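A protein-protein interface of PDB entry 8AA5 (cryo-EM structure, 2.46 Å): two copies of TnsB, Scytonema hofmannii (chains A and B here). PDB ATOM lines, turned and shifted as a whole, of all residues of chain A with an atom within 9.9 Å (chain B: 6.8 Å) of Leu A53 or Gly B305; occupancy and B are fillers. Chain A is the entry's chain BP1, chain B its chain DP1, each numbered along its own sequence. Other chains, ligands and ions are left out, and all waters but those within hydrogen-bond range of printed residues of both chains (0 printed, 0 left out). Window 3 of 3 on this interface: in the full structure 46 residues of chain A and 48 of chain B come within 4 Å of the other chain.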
ATOM      1  N   LYS A  45      -9.295  16.011   5.162  1.00  0.00           N
ATOM      2  CA  LYS A  45      -9.232  16.319   3.736  1.00  0.00           C
ATOM      3  C   LYS A  45      -8.620  15.163   2.950  1.00  0.00           C
ATOM      4  O   LYS A  45      -9.051  14.870   1.830  1.00  0.00           O
ATOM      5  CB  LYS A  45      -8.452  17.612   3.504  1.00  0.00           C
ATOM      6  CG  LYS A  45      -9.031  18.810   4.234  1.00  0.00           C
ATOM      7  CD  LYS A  45      -9.297  19.972   3.296  1.00  0.00           C
ATOM      8  CE  LYS A  45      -8.059  20.350   2.510  1.00  0.00           C
ATOM      9  NZ  LYS A  45      -8.116  21.760   2.041  1.00  0.00           N
ATOM     10  N   LEU A  46      -7.617  14.493   3.521  1.00  0.00           N
ATOM     11  CA  LEU A  46      -7.047  13.316   2.876  1.00  0.00           C
ATOM     12  C   LEU A  46      -8.072  12.195   2.777  1.00  0.00           C
ATOM     13  O   LEU A  46      -8.138  11.492   1.764  1.00  0.00           O
ATOM     14  CB  LEU A  46      -5.806  12.852   3.643  1.00  0.00           C
ATOM     15  CG  LEU A  46      -4.984  11.683   3.093  1.00  0.00           C
ATOM     16  CD1 LEU A  46      -3.518  11.893   3.417  1.00  0.00           C
ATOM     17  CD2 LEU A  46      -5.456  10.349   3.658  1.00  0.00           C
ATOM     18  N   GLU A  47      -8.874  12.011   3.827  1.00  0.00           N
ATOM     19  CA  GLU A  47      -9.933  11.006   3.776  1.00  0.00           C
ATOM     20  C   GLU A  47     -10.946  11.330   2.685  1.00  0.00           C
ATOM     21  O   GLU A  47     -11.385  10.438   1.946  1.00  0.00           O
ATOM     22  CB  GLU A  47     -10.625  10.901   5.135  1.00  0.00           C
ATOM     23  CG  GLU A  47     -11.598   9.741   5.246  1.00  0.00           C
ATOM     24  CD  GLU A  47     -10.898   8.403   5.387  1.00  0.00           C
ATOM     25  OE1 GLU A  47      -9.913   8.324   6.150  1.00  0.00           O
ATOM     26  OE2 GLU A  47     -11.333   7.432   4.735  1.00  0.00           O
ATOM     27  N   VAL A  48     -11.325  12.602   2.561  1.00  0.00           N
ATOM     28  CA  VAL A  48     -12.298  12.976   1.541  1.00  0.00           C
ATOM     29  C   VAL A  48     -11.700  12.816   0.144  1.00  0.00           C
ATOM     30  O   VAL A  48     -12.400  12.436  -0.802  1.00  0.00           O
ATOM     31  CB  VAL A  48     -12.832  14.401   1.796  1.00  0.00           C
ATOM     32  CG1 VAL A  48     -12.014  15.465   1.067  1.00  0.00           C
ATOM     33  CG2 VAL A  48     -14.297  14.487   1.423  1.00  0.00           C
ATOM     34  N   ILE A  49     -10.398  13.082  -0.007  1.00  0.00           N
ATOM     35  CA  ILE A  49      -9.769  12.904  -1.312  1.00  0.00           C
ATOM     36  C   ILE A  49      -9.637  11.423  -1.648  1.00  0.00           C
ATOM     37  O   ILE A  49      -9.702  11.039  -2.823  1.00  0.00           O
ATOM     38  CB  ILE A  49      -8.414  13.639  -1.371  1.00  0.00           C
ATOM     39  CG1 ILE A  49      -8.217  14.279  -2.744  1.00  0.00           C
ATOM     40  CG2 ILE A  49      -7.250  12.705  -1.077  1.00  0.00           C
ATOM     41  CD1 ILE A  49      -9.215  15.352  -3.061  1.00  0.00           C
ATOM     42  N   GLN A  50      -9.449  10.570  -0.637  1.00  0.00           N
ATOM     43  CA  GLN A  50      -9.450   9.130  -0.879  1.00  0.00           C
ATOM     44  C   GLN A  50     -10.833   8.652  -1.294  1.00  0.00           C
ATOM     45  O   GLN A  50     -10.962   7.798  -2.180  1.00  0.00           O
ATOM     46  CB  GLN A  50      -8.974   8.386   0.368  1.00  0.00           C
ATOM     47  CG  GLN A  50      -7.467   8.393   0.560  1.00  0.00           C
ATOM     48  CD  GLN A  50      -6.744   7.579  -0.495  1.00  0.00           C
ATOM     49  OE1 GLN A  50      -5.712   7.998  -1.019  1.00  0.00           O
ATOM     50  NE2 GLN A  50      -7.284   6.408  -0.812  1.00  0.00           N
ATOM     51  N   SER A  51     -11.878   9.190  -0.663  1.00  0.00           N
ATOM     52  CA  SER A  51     -13.239   8.872  -1.077  1.00  0.00           C
ATOM     53  C   SER A  51     -13.569   9.438  -2.453  1.00  0.00           C
ATOM     54  O   SER A  51     -14.485   8.937  -3.112  1.00  0.00           O
ATOM     55  CB  SER A  51     -14.241   9.392  -0.046  1.00  0.00           C
ATOM     56  OG  SER A  51     -14.121   8.690   1.180  1.00  0.00           O
ATOM     57  N   LEU A  52     -12.846  10.464  -2.897  1.00  0.00           N
ATOM     58  CA  LEU A  52     -13.064  11.075  -4.201  1.00  0.00           C
ATOM     59  C   LEU A  52     -12.173  10.500  -5.294  1.00  0.00           C
ATOM     60  O   LEU A  52     -12.254  10.953  -6.439  1.00  0.00           O
ATOM     61  CB  LEU A  52     -12.843  12.589  -4.112  1.00  0.00           C
ATOM     62  CG  LEU A  52     -14.091  13.470  -4.133  1.00  0.00           C
ATOM     63  CD1 LEU A  52     -14.907  13.266  -2.869  1.00  0.00           C
ATOM     64  CD2 LEU A  52     -13.708  14.929  -4.300  1.00  0.00           C
ATOM     65  N   LEU A  53     -11.328   9.520  -4.977  1.00  0.00           N
ATOM     66  CA  LEU A  53     -10.349   9.020  -5.933  1.00  0.00           C
ATOM     67  C   LEU A  53     -10.805   7.772  -6.676  1.00  0.00           C
ATOM     68  O   LEU A  53     -10.257   7.474  -7.744  1.00  0.00           O
ATOM     69  CB  LEU A  53      -9.020   8.728  -5.224  1.00  0.00           C
ATOM     70  CG  LEU A  53      -7.781   8.533  -6.102  1.00  0.00           C
ATOM     71  CD1 LEU A  53      -7.695   9.622  -7.161  1.00  0.00           C
ATOM     72  CD2 LEU A  53      -6.520   8.506  -5.254  1.00  0.00           C
ATOM     73  N   GLU A  54     -11.786   7.046  -6.152  1.00  0.00           N
ATOM     74  CA  GLU A  54     -12.254   5.842  -6.823  1.00  0.00           C
ATOM     75  C   GLU A  54     -12.877   6.205  -8.169  1.00  0.00           C
ATOM     76  O   GLU A  54     -13.746   7.086  -8.224  1.00  0.00           O
ATOM     77  CB  GLU A  54     -13.269   5.102  -5.953  1.00  0.00           C
ATOM     78  CG  GLU A  54     -13.793   3.819  -6.575  1.00  0.00           C
ATOM     79  CD  GLU A  54     -12.733   2.740  -6.664  1.00  0.00           C
ATOM     80  OE1 GLU A  54     -11.850   2.695  -5.782  1.00  0.00           O
ATOM     81  OE2 GLU A  54     -12.783   1.935  -7.618  1.00  0.00           O
ATOM     82  N   PRO A  55     -12.455   5.574  -9.264  1.00  0.00           N
ATOM     83  CA  PRO A  55     -13.033   5.902 -10.572  1.00  0.00           C
ATOM     84  C   PRO A  55     -14.529   5.625 -10.602  1.00  0.00           C
ATOM     85  O   PRO A  55     -15.010   4.640 -10.036  1.00  0.00           O
ATOM     86  CB  PRO A  55     -12.271   4.989 -11.539  1.00  0.00           C
ATOM     87  CG  PRO A  55     -11.009   4.631 -10.817  1.00  0.00           C
ATOM     88  CD  PRO A  55     -11.379   4.575  -9.367  1.00  0.00           C
ATOM     89  N   CYS A  56     -15.262   6.505 -11.274  1.00  0.00           N
ATOM     90  CA  CYS A  56     -16.715   6.418 -11.341  1.00  0.00           C
ATOM     91  C   CYS A  56     -17.187   7.271 -12.514  1.00  0.00           C
ATOM     92  O   CYS A  56     -16.389   7.679 -13.367  1.00  0.00           O
ATOM     93  CB  CYS A  56     -17.350   6.848 -10.016  1.00  0.00           C
ATOM     94  SG  CYS A  56     -16.721   8.408  -9.366  1.00  0.00           S
ATOM     95  N   ASP A  57     -18.488   7.541 -12.559  1.00  0.00           N
ATOM     96  CA  ASP A  57     -19.094   8.276 -13.658  1.00  0.00           C
ATOM     97  C   ASP A  57     -19.629   9.618 -13.177  1.00  0.00           C
ATOM     98  O   ASP A  57     -20.034   9.769 -12.021  1.00  0.00           O
ATOM     99  CB  ASP A  57     -20.225   7.472 -14.308  1.00  0.00           C
ATOM    100  CG  ASP A  57     -20.331   7.722 -15.799  1.00  0.00           C
ATOM    101  OD1 ASP A  57     -19.377   8.284 -16.379  1.00  0.00           O
ATOM    102  OD2 ASP A  57     -21.369   7.359 -16.391  1.00  0.00           O
ATOM    103  N   TYR A  61     -20.211  10.549  -9.779  1.00  0.00           N
ATOM    104  CA  TYR A  61     -19.083  11.324  -9.274  1.00  0.00           C
ATOM    105  C   TYR A  61     -19.557  12.619  -8.628  1.00  0.00           C
ATOM    106  O   TYR A  61     -19.060  13.011  -7.566  1.00  0.00           O
ATOM    107  CB  TYR A  61     -18.096  11.616 -10.407  1.00  0.00           C
ATOM    108  CG  TYR A  61     -17.237  12.839 -10.180  1.00  0.00           C
ATOM    109  CD1 TYR A  61     -16.069  12.761  -9.435  1.00  0.00           C
ATOM    110  CD2 TYR A  61     -17.589  14.070 -10.713  1.00  0.00           C
ATOM    111  CE1 TYR A  61     -15.283  13.870  -9.222  1.00  0.00           C
ATOM    112  CE2 TYR A  61     -16.809  15.185 -10.502  1.00  0.00           C
ATOM    113  CZ  TYR A  61     -15.657  15.081  -9.760  1.00  0.00           C
ATOM    114  OH  TYR A  61     -14.875  16.193  -9.553  1.00  0.00           O
ATOM    115  N   LYS A  64     -20.883  12.242  -4.844  1.00  0.00           N
ATOM    116  CA  LYS A  64     -19.852  12.286  -3.816  1.00  0.00           C
ATOM    117  C   LYS A  64     -19.092  13.605  -3.827  1.00  0.00           C
ATOM    118  O   LYS A  64     -18.542  13.989  -2.794  1.00  0.00           O
ATOM    119  CB  LYS A  64     -18.888  11.107  -3.968  1.00  0.00           C
ATOM    120  CG  LYS A  64     -18.324  10.909  -5.360  1.00  0.00           C
ATOM    121  CD  LYS A  64     -16.849  11.265  -5.407  1.00  0.00           C
ATOM    122  CE  LYS A  64     -16.196  10.719  -6.663  1.00  0.00           C
ATOM    123  NZ  LYS A  64     -14.869  11.338  -6.920  1.00  0.00           N
ATOM    124  N   LEU A  65     -19.074  14.322  -4.953  1.00  0.00           N
ATOM    125  CA  LEU A  65     -18.488  15.660  -4.961  1.00  0.00           C
ATOM    126  C   LEU A  65     -19.244  16.594  -4.019  1.00  0.00           C
ATOM    127  O   LEU A  65     -18.645  17.246  -3.150  1.00  0.00           O
ATOM    128  CB  LEU A  65     -18.484  16.211  -6.387  1.00  0.00           C
ATOM    129  CG  LEU A  65     -17.772  17.539  -6.638  1.00  0.00           C
ATOM    130  CD1 LEU A  65     -16.379  17.508  -6.047  1.00  0.00           C
ATOM    131  CD2 LEU A  65     -17.710  17.832  -8.128  1.00  0.00           C
ATOM    132  N   ALA A  68     -18.761  15.571  -0.435  1.00  0.00           N
ATOM    133  CA  ALA A  68     -17.529  16.150   0.088  1.00  0.00           C
ATOM    134  C   ALA A  68     -17.721  17.618   0.437  1.00  0.00           C
ATOM    135  O   ALA A  68     -17.213  18.096   1.457  1.00  0.00           O
ATOM    136  CB  ALA A  68     -16.405  15.990  -0.933  1.00  0.00           C
ATOM    137  N   VAL A  79     -14.289  22.318  -3.328  1.00  0.00           N
ATOM    138  CA  VAL A  79     -13.772  20.967  -3.527  1.00  0.00           C
ATOM    139  C   VAL A  79     -13.135  20.834  -4.906  1.00  0.00           C
ATOM    140  O   VAL A  79     -12.171  20.079  -5.084  1.00  0.00           O
ATOM    141  CB  VAL A  79     -14.890  19.930  -3.313  1.00  0.00           C
ATOM    142  CG1 VAL A  79     -14.310  18.528  -3.285  1.00  0.00           C
ATOM    143  CG2 VAL A  79     -15.627  20.218  -2.022  1.00  0.00           C
ATOM    144  N   VAL A  83      -9.342  19.501  -5.352  1.00  0.00           N
ATOM    145  CA  VAL A  83      -8.859  18.413  -6.197  1.00  0.00           C
ATOM    146  C   VAL A  83      -7.880  18.941  -7.241  1.00  0.00           C
ATOM    147  O   VAL A  83      -6.903  18.266  -7.587  1.00  0.00           O
ATOM    148  CB  VAL A  83     -10.033  17.642  -6.831  1.00  0.00           C
ATOM    149  CG1 VAL A  83     -10.920  17.053  -5.747  1.00  0.00           C
ATOM    150  CG2 VAL A  83     -10.842  18.521  -7.768  1.00  0.00           C
ATOM    151  N   TRP A  86      -4.636  19.454  -5.421  1.00  0.00           N
ATOM    152  CA  TRP A  86      -4.122  18.144  -5.037  1.00  0.00           C
ATOM    153  C   TRP A  86      -3.479  17.434  -6.221  1.00  0.00           C
ATOM    154  O   TRP A  86      -2.436  16.789  -6.071  1.00  0.00           O
ATOM    155  CB  TRP A  86      -5.250  17.305  -4.432  1.00  0.00           C
ATOM    156  CG  TRP A  86      -5.090  15.819  -4.578  1.00  0.00           C
ATOM    157  CD1 TRP A  86      -4.529  14.967  -3.676  1.00  0.00           C
ATOM    158  CD2 TRP A  86      -5.535  15.008  -5.671  1.00  0.00           C
ATOM    159  NE1 TRP A  86      -4.577  13.680  -4.147  1.00  0.00           N
ATOM    160  CE2 TRP A  86      -5.191  13.677  -5.370  1.00  0.00           C
ATOM    161  CE3 TRP A  86      -6.185  15.278  -6.879  1.00  0.00           C
ATOM    162  CZ2 TRP A  86      -5.474  12.622  -6.231  1.00  0.00           C
ATOM    163  CZ3 TRP A  86      -6.460  14.233  -7.731  1.00  0.00           C
ATOM    164  CH2 TRP A  86      -6.107  12.919  -7.405  1.00  0.00           C
ATOM    165  N   GLU A  87      -4.084  17.533  -7.406  1.00  0.00           N
ATOM    166  CA  GLU A  87      -3.490  16.884  -8.568  1.00  0.00           C
ATOM    167  C   GLU A  87      -2.307  17.668  -9.122  1.00  0.00           C
ATOM    168  O   GLU A  87      -1.396  17.068  -9.704  1.00  0.00           O
ATOM    169  CB  GLU A  87      -4.542  16.663  -9.660  1.00  0.00           C
ATOM    170  CG  GLU A  87      -5.066  17.921 -10.330  1.00  0.00           C
ATOM    171  CD  GLU A  87      -4.296  18.276 -11.585  1.00  0.00           C
ATOM    172  OE1 GLU A  87      -3.524  17.423 -12.070  1.00  0.00           O
ATOM    173  OE2 GLU A  87      -4.466  19.406 -12.089  1.00  0.00           O
ATOM    174  N   GLY A  90       0.089  17.539  -5.347  1.00  0.00           N
ATOM    175  CA  GLY A  90       0.192  16.376  -4.488  1.00  0.00           C
ATOM    176  C   GLY A  90      -0.455  16.607  -3.142  1.00  0.00           C
ATOM    177  O   GLY A  90      -1.411  17.378  -3.028  1.00  0.00           O
ATOM    178  N   LEU A  91       0.062  15.945  -2.107  1.00  0.00           N
ATOM    179  CA  LEU A  91      -0.437  16.169  -0.757  1.00  0.00           C
ATOM    180  C   LEU A  91       0.053  17.483  -0.171  1.00  0.00           C
ATOM    181  O   LEU A  91      -0.424  17.891   0.893  1.00  0.00           O
ATOM    182  CB  LEU A  91      -0.032  15.011   0.150  1.00  0.00           C
ATOM    183  CG  LEU A  91      -0.682  13.664  -0.155  1.00  0.00           C
ATOM    184  CD1 LEU A  91      -0.881  12.919   1.129  1.00  0.00           C
ATOM    185  CD2 LEU A  91      -2.011  13.836  -0.873  1.00  0.00           C
ATOM    186  N   LEU A  94      -2.744  19.718  -0.604  1.00  0.00           N
ATOM    187  CA  LEU A  94      -3.834  19.378   0.302  1.00  0.00           C
ATOM    188  C   LEU A  94      -3.914  20.362   1.461  1.00  0.00           C
ATOM    189  O   LEU A  94      -5.005  20.808   1.833  1.00  0.00           O
ATOM    190  CB  LEU A  94      -3.653  17.952   0.816  1.00  0.00           C
ATOM    191  CG  LEU A  94      -4.812  17.309   1.572  1.00  0.00           C
ATOM    192  CD1 LEU A  94      -4.972  15.861   1.150  1.00  0.00           C
ATOM    193  CD2 LEU A  94      -4.573  17.403   3.062  1.00  0.00           C
ATOM    194  N   LYS B 280       2.414   1.877 -12.889  1.00  0.00           N
ATOM    195  CA  LYS B 280       1.579   2.254 -11.762  1.00  0.00           C
ATOM    196  C   LYS B 280       0.221   1.571 -11.876  1.00  0.00           C
ATOM    197  O   LYS B 280      -0.385   1.572 -12.955  1.00  0.00           O
ATOM    198  CB  LYS B 280       1.432   3.785 -11.746  1.00  0.00           C
ATOM    199  CG  LYS B 280       1.266   4.458 -10.392  1.00  0.00           C
ATOM    200  CD  LYS B 280      -0.119   4.227  -9.837  1.00  0.00           C
ATOM    201  CE  LYS B 280      -1.094   5.188 -10.497  1.00  0.00           C
ATOM    202  NZ  LYS B 280      -2.407   5.250  -9.814  1.00  0.00           N
ATOM    203  N   PRO B 281      -0.277   0.974 -10.797  1.00  0.00           N
ATOM    204  CA  PRO B 281      -1.560   0.271 -10.856  1.00  0.00           C
ATOM    205  C   PRO B 281      -2.751   1.193 -10.625  1.00  0.00           C
ATOM    206  O   PRO B 281      -2.635   2.290 -10.074  1.00  0.00           O
ATOM    207  CB  PRO B 281      -1.437  -0.739  -9.709  1.00  0.00           C
ATOM    208  CG  PRO B 281      -0.652   0.001  -8.697  1.00  0.00           C
ATOM    209  CD  PRO B 281       0.356   0.828  -9.475  1.00  0.00           C
ATOM    210  N   GLU B 282      -3.919   0.715 -11.062  1.00  0.00           N
ATOM    211  CA  GLU B 282      -5.156   1.430 -10.770  1.00  0.00           C
ATOM    212  C   GLU B 282      -5.567   1.248  -9.315  1.00  0.00           C
ATOM    213  O   GLU B 282      -5.983   2.207  -8.657  1.00  0.00           O
ATOM    214  CB  GLU B 282      -6.269   0.965 -11.708  1.00  0.00           C
ATOM    215  CG  GLU B 282      -6.637   1.972 -12.787  1.00  0.00           C
ATOM    216  CD  GLU B 282      -5.609   2.051 -13.902  1.00  0.00           C
ATOM    217  OE1 GLU B 282      -4.646   1.255 -13.892  1.00  0.00           O
ATOM    218  OE2 GLU B 282      -5.766   2.911 -14.793  1.00  0.00           O
ATOM    219  N   SER B 298      -2.441   5.174   2.491  1.00  0.00           N
ATOM    220  CA  SER B 298      -3.329   6.061   1.751  1.00  0.00           C
ATOM    221  C   SER B 298      -2.620   7.341   1.338  1.00  0.00           C
ATOM    222  O   SER B 298      -2.990   7.960   0.335  1.00  0.00           O
ATOM    223  CB  SER B 298      -4.565   6.384   2.589  1.00  0.00           C
ATOM    224  OG  SER B 298      -4.198   6.836   3.881  1.00  0.00           O
ATOM    225  N   ILE B 300       0.601   7.652   0.231  1.00  0.00           N
ATOM    226  CA  ILE B 300       1.232   7.382  -1.058  1.00  0.00           C
ATOM    227  C   ILE B 300       0.180   7.120  -2.123  1.00  0.00           C
ATOM    228  O   ILE B 300       0.374   7.469  -3.293  1.00  0.00           O
ATOM    229  CB  ILE B 300       2.248   6.221  -0.995  1.00  0.00           C
ATOM    230  CG1 ILE B 300       3.097   6.240   0.281  1.00  0.00           C
ATOM    231  CG2 ILE B 300       3.156   6.243  -2.212  1.00  0.00           C
ATOM    232  CD1 ILE B 300       2.504   5.517   1.451  1.00  0.00           C
ATOM    233  N   GLY B 301      -0.935   6.489  -1.753  1.00  0.00           N
ATOM    234  CA  GLY B 301      -1.998   6.273  -2.722  1.00  0.00           C
ATOM    235  C   GLY B 301      -2.516   7.570  -3.313  1.00  0.00           C
ATOM    236  O   GLY B 301      -2.727   7.674  -4.524  1.00  0.00           O
ATOM    237  N   ALA B 302      -2.718   8.580  -2.466  1.00  0.00           N
ATOM    238  CA  ALA B 302      -3.154   9.883  -2.954  1.00  0.00           C
ATOM    239  C   ALA B 302      -2.031  10.623  -3.667  1.00  0.00           C
ATOM    240  O   ALA B 302      -2.289  11.385  -4.604  1.00  0.00           O
ATOM    241  CB  ALA B 302      -3.693  10.720  -1.797  1.00  0.00           C
ATOM    242  N   GLN B 303      -0.783  10.414  -3.242  1.00  0.00           N
ATOM    243  CA  GLN B 303       0.334  11.137  -3.841  1.00  0.00           C
ATOM    244  C   GLN B 303       0.656  10.628  -5.242  1.00  0.00           C
ATOM    245  O   GLN B 303       1.075  11.411  -6.101  1.00  0.00           O
ATOM    246  CB  GLN B 303       1.559  11.034  -2.927  1.00  0.00           C
ATOM    247  CG  GLN B 303       2.868  11.447  -3.565  1.00  0.00           C
ATOM    248  CD  GLN B 303       2.928  12.927  -3.855  1.00  0.00           C
ATOM    249  OE1 GLN B 303       2.981  13.342  -5.010  1.00  0.00           O
ATOM    250  NE2 GLN B 303       2.922  13.735  -2.804  1.00  0.00           N
ATOM    251  N   LEU B 304       0.461   9.335  -5.496  1.00  0.00           N
ATOM    252  CA  LEU B 304       0.762   8.747  -6.795  1.00  0.00           C
ATOM    253  C   LEU B 304      -0.455   8.616  -7.698  1.00  0.00           C
ATOM    254  O   LEU B 304      -0.311   8.691  -8.923  1.00  0.00           O
ATOM    255  CB  LEU B 304       1.403   7.366  -6.620  1.00  0.00           C
ATOM    256  CG  LEU B 304       2.660   7.289  -5.753  1.00  0.00           C
ATOM    257  CD1 LEU B 304       3.254   5.895  -5.813  1.00  0.00           C
ATOM    258  CD2 LEU B 304       3.681   8.329  -6.190  1.00  0.00           C
ATOM    259  N   GLY B 305      -1.642   8.419  -7.132  1.00  0.00           N
ATOM    260  CA  GLY B 305      -2.879   8.368  -7.889  1.00  0.00           C
ATOM    261  C   GLY B 305      -3.718   7.132  -7.648  1.00  0.00           C
ATOM    262  O   GLY B 305      -4.914   7.137  -7.974  1.00  0.00           O
ATOM    263  N   PHE B 306      -3.142   6.073  -7.091  1.00  0.00           N
ATOM    264  CA  PHE B 306      -3.854   4.816  -6.936  1.00  0.00           C
ATOM    265  C   PHE B 306      -4.711   4.833  -5.675  1.00  0.00           C
ATOM    266  O   PHE B 306      -4.653   5.752  -4.857  1.00  0.00           O
ATOM    267  CB  PHE B 306      -2.852   3.648  -6.989  1.00  0.00           C
ATOM    268  CG  PHE B 306      -2.075   3.394  -5.707  1.00  0.00           C
ATOM    269  CD1 PHE B 306      -2.692   3.081  -4.502  1.00  0.00           C
ATOM    270  CD2 PHE B 306      -0.697   3.493  -5.724  1.00  0.00           C
ATOM    271  CE1 PHE B 306      -1.957   2.863  -3.360  1.00  0.00           C
ATOM    272  CE2 PHE B 306       0.040   3.280  -4.586  1.00  0.00           C
ATOM    273  CZ  PHE B 306      -0.589   2.964  -3.403  1.00  0.00           C
ATOM    274  N   VAL B 307      -5.520   3.790  -5.527  1.00  0.00           N
ATOM    275  CA  VAL B 307      -6.412   3.627  -4.387  1.00  0.00           C
ATOM    276  C   VAL B 307      -5.901   2.466  -3.550  1.00  0.00           C
ATOM    277  O   VAL B 307      -5.721   1.354  -4.062  1.00  0.00           O
ATOM    278  CB  VAL B 307      -7.864   3.387  -4.838  1.00  0.00           C
ATOM    279  CG1 VAL B 307      -8.836   3.756  -3.727  1.00  0.00           C
ATOM    280  CG2 VAL B 307      -8.161   4.176  -6.103  1.00  0.00           C
ATOM    281  N   CYS B 308      -5.666   2.721  -2.269  1.00  0.00           N
ATOM    282  CA  CYS B 308      -5.148   1.716  -1.356  1.00  0.00           C
ATOM    283  C   CYS B 308      -6.285   1.120  -0.540  1.00  0.00           C
ATOM    284  O   CYS B 308      -7.201   1.832  -0.119  1.00  0.00           O
ATOM    285  CB  CYS B 308      -4.094   2.314  -0.423  1.00  0.00           C
ATOM    286  SG  CYS B 308      -3.782   1.336   1.063  1.00  0.00           S
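O of Gly B301 sits at hydrogen-bond distance from N of Phe B306, at 3.1 Å. The backbone carbonyl oxygen of Glu A54 sits at hydrogen-bond distance from the side-chain sulfur of Cys A56 (3.4 Å).
Ser B298 touches Leu A46. Gly B301 touches Gln A50 (C to OE1, 3.96 Å). Leu A53 touches Gly B301 (CD2 to O, 3.95 Å). CD2 of Leu A53 touches O of Gly B305 (3.4 Å). O of Phe B306 touches CD2 of Leu A53, 3.4 Å away. Glu A54 touches Val B307. Leu A91 touches Ala B302. NE2 of Gln B303 touches N of Leu A91 (3.7 Å).
Of the 24 printed residues of chain A, 6 touch a printed residue of chain B. Hydrophobic or aromatic side chains of chain A within 4 Å of the printed part of chain B: Leu A46, Leu A53, Trp A86 and Leu A91. Printed residues of chain B that touch a printed residue of chain A: Ser B298, Gly B301, Ala B302, Gln B303, Gly B305, Phe B306 and Val B307. Hydrophobic or aromatic side chains of chain B that line the printed part of chain A: Ala B302 and Val B307. Among the printed residues, no Asp or Glu carboxylate lies within 4 Å of a Lys or Arg side-chain nitrogen of the other chain.
Of chain B, only Gly B301, Gly B305 and Phe B306 come within 4 Å of Leu A53. Gly B305 touches just one residue of chain A: Leu A53 (3.4 Å). Of chain A, only Gln A50 (3.96 Å) and Leu A53 (3.95 Å) come within 4 Å of Gly B301. Of the printed residues of chain B, Trp A86 touches Ala B302 (3.3 Å). Printed residues of chain A within 4 Å of Val B307: Glu A54 (3.8 Å). Of the printed residues of chain A, Gln B303 touches Leu A91 (3.7 Å). Lys B280 touches none of the printed residues of chain A. Ile A49 touches none of the printed residues of chain B.
OE1 of Gln A50 is in hydrogen-bond range of N of Ala B302 (3.4 Å). OE1 of Gln A50 lies close to O of Ser B298 (3.0 Å). The indole nitrogen of Trp A86 sits at hydrogen-bond distance from the backbone carbonyl oxygen of Ala B302, 3.3 Å away.
No position is printed for both chains.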
